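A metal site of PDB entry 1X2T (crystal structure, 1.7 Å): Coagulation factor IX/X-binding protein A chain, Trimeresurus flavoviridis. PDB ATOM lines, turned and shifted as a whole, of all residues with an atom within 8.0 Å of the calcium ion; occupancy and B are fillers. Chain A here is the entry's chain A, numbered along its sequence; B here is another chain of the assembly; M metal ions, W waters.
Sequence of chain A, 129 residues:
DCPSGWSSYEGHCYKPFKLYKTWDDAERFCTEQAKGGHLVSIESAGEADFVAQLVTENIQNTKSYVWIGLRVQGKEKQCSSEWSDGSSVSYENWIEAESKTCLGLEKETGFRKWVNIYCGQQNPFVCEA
Glu 43 touches the calcium ion.
Four residues have an atom within 4 Å of the calcium ion: Ser 41, Glu 43, Glu 47 and Glu 128.
The nearest printed residue that does not touch the calcium ion is Tyr 14 (4.1 Å).
Water W1 bridges the side-chain carboxylate of Glu 47 (3.2 Å) and a ring nitrogen (ND1) of His 12 (3.4 Å).
The side-chain hydroxyl of Ser 41 sits close to the side-chain carboxylate of Glu 43, at 3.3 Å.
ND2 of Asn 81 of chain B sits close to OG of Ser 41, at 3.1 Å.
The side-chain hydroxyl (OH) of Tyr 9 is in hydrogen-bond range of the backbone NH (N) of Glu 47 (3.3 Å).
OE1 of Glu 47 sits at hydrogen-bond distance from N of Glu 43 (2.9 Å).
The side-chain carboxylate (OE2) of Glu 47 lies close to the side-chain hydroxyl (OH) of Tyr 14, 2.5 Å away.
The backbone NH (N) of Glu 47 lies within hydrogen-bond range of the side-chain hydroxyl (OG) of Ser 44, 3.2 Å away.
The side-chain carboxylate (OE2) of Glu 128 lies close to a ring nitrogen (ND1) of His 12, at 2.8 Å.
OH of Tyr 14 sits close to OE2 of Glu 128.
The calcium ion is bound by OG of Ser 41 (2.3 Å), OE2 of Glu 128 (2.3 Å), OE2 of Glu 47 (2.5 Å), O of Ser 41 (2.6 Å), water W1 (2.6 Å) and OE1 of Glu 128 (2.7 Å).
The calcium ion has six donor atoms within binding distance.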
ATOM      1  N   TYR A   9      13.620   0.009  23.008  1.00  0.00           N
ATOM      2  CA  TYR A   9      14.586  -1.037  23.311  1.00  0.00           C
ATOM      3  C   TYR A   9      14.356  -2.223  22.379  1.00  0.00           C
ATOM      4  O   TYR A   9      13.236  -2.727  22.271  1.00  0.00           O
ATOM      5  CB  TYR A   9      14.456  -1.506  24.764  1.00  0.00           C
ATOM      6  CG  TYR A   9      15.368  -2.684  25.075  1.00  0.00           C
ATOM      7  CD1 TYR A   9      16.741  -2.499  25.215  1.00  0.00           C
ATOM      8  CD2 TYR A   9      14.866  -3.981  25.145  1.00  0.00           C
ATOM      9  CE1 TYR A   9      17.593  -3.572  25.424  1.00  0.00           C
ATOM     10  CE2 TYR A   9      15.715  -5.068  25.345  1.00  0.00           C
ATOM     11  CZ  TYR A   9      17.073  -4.858  25.482  1.00  0.00           C
ATOM     12  OH  TYR A   9      17.920  -5.923  25.679  1.00  0.00           O
ATOM     13  N   HIS A  12      11.220  -2.460  20.276  1.00  0.00           N
ATOM     14  CA  HIS A  12       9.914  -2.355  20.945  1.00  0.00           C
ATOM     15  C   HIS A  12       9.790  -1.028  21.690  1.00  0.00           C
ATOM     16  O   HIS A  12      10.784  -0.330  21.888  1.00  0.00           O
ATOM     17  CB  HIS A  12       9.718  -3.516  21.917  1.00  0.00           C
ATOM     18  CG  HIS A  12       9.585  -4.853  21.266  1.00  0.00           C
ATOM     19  ND1 HIS A  12       9.225  -5.988  21.947  1.00  0.00           N
ATOM     20  CD2 HIS A  12       9.765  -5.233  19.970  1.00  0.00           C
ATOM     21  CE1 HIS A  12       9.189  -7.017  21.116  1.00  0.00           C
ATOM     22  NE2 HIS A  12       9.519  -6.582  19.915  1.00  0.00           N
ATOM     23  N   CYS A  13       8.578  -0.693  22.091  1.00  0.00           N
ATOM     24  CA  CYS A  13       8.322   0.558  22.816  1.00  0.00           C
ATOM     25  C   CYS A  13       7.772   0.259  24.208  1.00  0.00           C
ATOM     26  O   CYS A  13       6.896  -0.579  24.370  1.00  0.00           O
ATOM     27  CB  CYS A  13       7.343   1.431  22.045  1.00  0.00           C
ATOM     28  SG  CYS A  13       7.936   1.831  20.359  1.00  0.00           S
ATOM     29  N   TYR A  14       8.300   0.956  25.214  1.00  0.00           N
ATOM     30  CA  TYR A  14       7.870   0.741  26.592  1.00  0.00           C
ATOM     31  C   TYR A  14       7.472   2.050  27.254  1.00  0.00           C
ATOM     32  O   TYR A  14       8.013   3.106  26.928  1.00  0.00           O
ATOM     33  CB  TYR A  14       9.028   0.138  27.401  1.00  0.00           C
ATOM     34  CG  TYR A  14       9.615  -1.121  26.792  1.00  0.00           C
ATOM     35  CD1 TYR A  14      10.355  -1.075  25.611  1.00  0.00           C
ATOM     36  CD2 TYR A  14       9.425  -2.373  27.397  1.00  0.00           C
ATOM     37  CE1 TYR A  14      10.895  -2.234  25.051  1.00  0.00           C
ATOM     38  CE2 TYR A  14       9.948  -3.537  26.841  1.00  0.00           C
ATOM     39  CZ  TYR A  14      10.691  -3.454  25.665  1.00  0.00           C
ATOM     40  OH  TYR A  14      11.221  -4.594  25.113  1.00  0.00           O
ATOM     41  N   LEU A  39       1.026  -5.624  29.237  1.00  0.00           N
ATOM     42  CA  LEU A  39       1.922  -5.373  30.351  1.00  0.00           C
ATOM     43  C   LEU A  39       3.258  -5.889  29.813  1.00  0.00           C
ATOM     44  O   LEU A  39       3.279  -6.817  29.006  1.00  0.00           O
ATOM     45  CB  LEU A  39       1.517  -6.168  31.581  1.00  0.00           C
ATOM     46  CG  LEU A  39       0.436  -5.510  32.427  1.00  0.00           C
ATOM     47  CD1 LEU A  39      -0.051  -6.490  33.480  1.00  0.00           C
ATOM     48  CD2 LEU A  39       1.011  -4.250  33.082  1.00  0.00           C
ATOM     49  N   VAL A  40       4.354  -5.304  30.280  1.00  0.00           N
ATOM     50  CA  VAL A  40       5.682  -5.683  29.818  1.00  0.00           C
ATOM     51  C   VAL A  40       6.054  -7.153  29.969  1.00  0.00           C
ATOM     52  O   VAL A  40       5.764  -7.785  30.996  1.00  0.00           O
ATOM     53  CB  VAL A  40       6.786  -4.805  30.510  1.00  0.00           C
ATOM     54  CG1 VAL A  40       6.837  -5.092  32.014  1.00  0.00           C
ATOM     55  CG2 VAL A  40       8.153  -5.050  29.858  1.00  0.00           C
ATOM     56  N   SER A  41       6.682  -7.701  28.929  1.00  0.00           N
ATOM     57  CA  SER A  41       7.147  -9.079  28.931  1.00  0.00           C
ATOM     58  C   SER A  41       8.668  -8.981  28.997  1.00  0.00           C
ATOM     59  O   SER A  41       9.279  -8.235  28.240  1.00  0.00           O
ATOM     60  CB  SER A  41       6.715  -9.818  27.660  1.00  0.00           C
ATOM     61  OG  SER A  41       7.026  -9.056  26.511  1.00  0.00           O
ATOM     62  N   ILE A  42       9.274  -9.716  29.917  1.00  0.00           N
ATOM     63  CA  ILE A  42      10.724  -9.691  30.090  1.00  0.00           C
ATOM     64  C   ILE A  42      11.238 -11.050  29.626  1.00  0.00           C
ATOM     65  O   ILE A  42      11.231 -12.028  30.369  1.00  0.00           O
ATOM     66  CB  ILE A  42      11.048  -9.421  31.567  1.00  0.00           C
ATOM     67  CG1 ILE A  42      10.484  -8.043  31.948  1.00  0.00           C
ATOM     68  CG2 ILE A  42      12.561  -9.450  31.785  1.00  0.00           C
ATOM     69  CD1 ILE A  42      10.729  -7.620  33.379  1.00  0.00           C
ATOM     70  N   GLU A  43      11.674 -11.075  28.374  1.00  0.00           N
ATOM     71  CA  GLU A  43      12.119 -12.294  27.734  1.00  0.00           C
ATOM     72  C   GLU A  43      13.612 -12.575  27.644  1.00  0.00           C
ATOM     73  O   GLU A  43      14.021 -13.556  27.032  1.00  0.00           O
ATOM     74  CB  GLU A  43      11.490 -12.357  26.335  1.00  0.00           C
ATOM     75  CG  GLU A  43       9.972 -12.249  26.395  1.00  0.00           C
ATOM     76  CD  GLU A  43       9.341 -12.315  25.013  1.00  0.00           C
ATOM     77  OE1 GLU A  43       9.673 -13.256  24.253  1.00  0.00           O
ATOM     78  OE2 GLU A  43       8.516 -11.444  24.705  1.00  0.00           O
ATOM     79  N   SER A  44      14.434 -11.721  28.233  1.00  0.00           N
ATOM     80  CA  SER A  44      15.872 -11.922  28.218  1.00  0.00           C
ATOM     81  C   SER A  44      16.526 -11.083  29.299  1.00  0.00           C
ATOM     82  O   SER A  44      15.895 -10.166  29.837  1.00  0.00           O
ATOM     83  CB  SER A  44      16.470 -11.554  26.850  1.00  0.00           C
ATOM     84  OG  SER A  44      16.404 -10.160  26.627  1.00  0.00           O
ATOM     85  N   GLU A  47      16.638  -7.437  28.290  1.00  0.00           N
ATOM     86  CA  GLU A  47      15.381  -6.736  28.449  1.00  0.00           C
ATOM     87  C   GLU A  47      15.146  -6.486  29.934  1.00  0.00           C
ATOM     88  O   GLU A  47      14.634  -5.440  30.317  1.00  0.00           O
ATOM     89  CB  GLU A  47      14.223  -7.533  27.833  1.00  0.00           C
ATOM     90  CG  GLU A  47      12.900  -6.766  27.767  1.00  0.00           C
ATOM     91  CD  GLU A  47      11.878  -7.442  26.886  1.00  0.00           C
ATOM     92  OE1 GLU A  47      11.956  -8.681  26.721  1.00  0.00           O
ATOM     93  OE2 GLU A  47      10.977  -6.744  26.362  1.00  0.00           O
ATOM     94  N   VAL A  51      14.465  -2.766  31.472  1.00  0.00           N
ATOM     95  CA  VAL A  51      13.257  -2.485  32.241  1.00  0.00           C
ATOM     96  C   VAL A  51      13.574  -2.066  33.684  1.00  0.00           C
ATOM     97  O   VAL A  51      12.923  -1.168  34.218  1.00  0.00           O
ATOM     98  CB  VAL A  51      12.306  -3.710  32.271  1.00  0.00           C
ATOM     99  CG1 VAL A  51      11.115  -3.419  33.201  1.00  0.00           C
ATOM    100  CG2 VAL A  51      11.806  -4.018  30.863  1.00  0.00           C
ATOM    101  N   GLU A 128       4.062  -2.364  27.147  1.00  0.00           N
ATOM    102  CA  GLU A 128       4.962  -2.620  26.022  1.00  0.00           C
ATOM    103  C   GLU A 128       4.160  -2.881  24.746  1.00  0.00           C
ATOM    104  O   GLU A 128       3.088  -3.477  24.782  1.00  0.00           O
ATOM    105  CB  GLU A 128       5.842  -3.836  26.331  1.00  0.00           C
ATOM    106  CG  GLU A 128       6.805  -4.232  25.223  1.00  0.00           C
ATOM    107  CD  GLU A 128       7.537  -5.528  25.515  1.00  0.00           C
ATOM    108  OE1 GLU A 128       7.505  -5.984  26.674  1.00  0.00           O
ATOM    109  OE2 GLU A 128       8.161  -6.098  24.588  1.00  0.00           O
ATOM    110  N   ALA A 129       4.699  -2.423  23.624  1.00  0.00           N
ATOM    111  CA  ALA A 129       4.048  -2.622  22.334  1.00  0.00           C
ATOM    112  C   ALA A 129       5.105  -2.738  21.234  1.00  0.00           C
ATOM    113  O   ALA A 129       6.261  -2.342  21.489  1.00  0.00           O
ATOM    114  CB  ALA A 129       3.113  -1.465  22.036  1.00  0.00           C
ATOM    115  OXT ALA A 129       4.763  -3.214  20.133  1.00  0.00           O
ATOM    116  N   TRP B  79       2.766 -15.312  29.693  1.00  0.00           N
ATOM    117  CA  TRP B  79       2.932 -13.879  29.460  1.00  0.00           C
ATOM    118  C   TRP B  79       1.647 -13.385  28.813  1.00  0.00           C
ATOM    119  O   TRP B  79       1.101 -14.047  27.927  1.00  0.00           O
ATOM    120  CB  TRP B  79       4.109 -13.607  28.520  1.00  0.00           C
ATOM    121  CG  TRP B  79       5.445 -13.799  29.146  1.00  0.00           C
ATOM    122  CD1 TRP B  79       6.323 -14.833  28.912  1.00  0.00           C
ATOM    123  CD2 TRP B  79       6.084 -12.936  30.089  1.00  0.00           C
ATOM    124  NE1 TRP B  79       7.473 -14.654  29.664  1.00  0.00           N
ATOM    125  CE2 TRP B  79       7.341 -13.504  30.403  1.00  0.00           C
ATOM    126  CE3 TRP B  79       5.708 -11.734  30.715  1.00  0.00           C
ATOM    127  CZ2 TRP B  79       8.229 -12.908  31.297  1.00  0.00           C
ATOM    128  CZ3 TRP B  79       6.593 -11.147  31.614  1.00  0.00           C
ATOM    129  CH2 TRP B  79       7.838 -11.738  31.900  1.00  0.00           C
ATOM    130  N   ASN B  81       1.248 -11.192  26.644  1.00  0.00           N
ATOM    131  CA  ASN B  81       1.447 -10.886  25.234  1.00  0.00           C
ATOM    132  C   ASN B  81       1.596 -12.169  24.409  1.00  0.00           C
ATOM    133  O   ASN B  81       1.919 -12.112  23.223  1.00  0.00           O
ATOM    134  CB  ASN B  81       2.695 -10.009  25.056  1.00  0.00           C
ATOM    135  CG  ASN B  81       3.987 -10.808  25.133  1.00  0.00           C
ATOM    136  OD1 ASN B  81       4.066 -11.828  25.802  1.00  0.00           O
ATOM    137  ND2 ASN B  81       5.029 -10.320  24.455  1.00  0.00           N
ATOM    138  N   ALA B  83       3.837 -14.432  24.611  1.00  0.00           N
ATOM    139  CA  ALA B  83       5.215 -14.893  24.423  1.00  0.00           C
ATOM    140  C   ALA B  83       5.387 -16.156  25.244  1.00  0.00           C
ATOM    141  O   ALA B  83       4.788 -16.293  26.315  1.00  0.00           O
ATOM    142  CB  ALA B  83       6.208 -13.827  24.873  1.00  0.00           C
HETATM  143 CA    CA M   1       8.955  -7.990  25.720  1.00  0.00          CA
HETATM  144  O   HOH W   1      10.695  -8.457  23.786  1.00  0.00           O
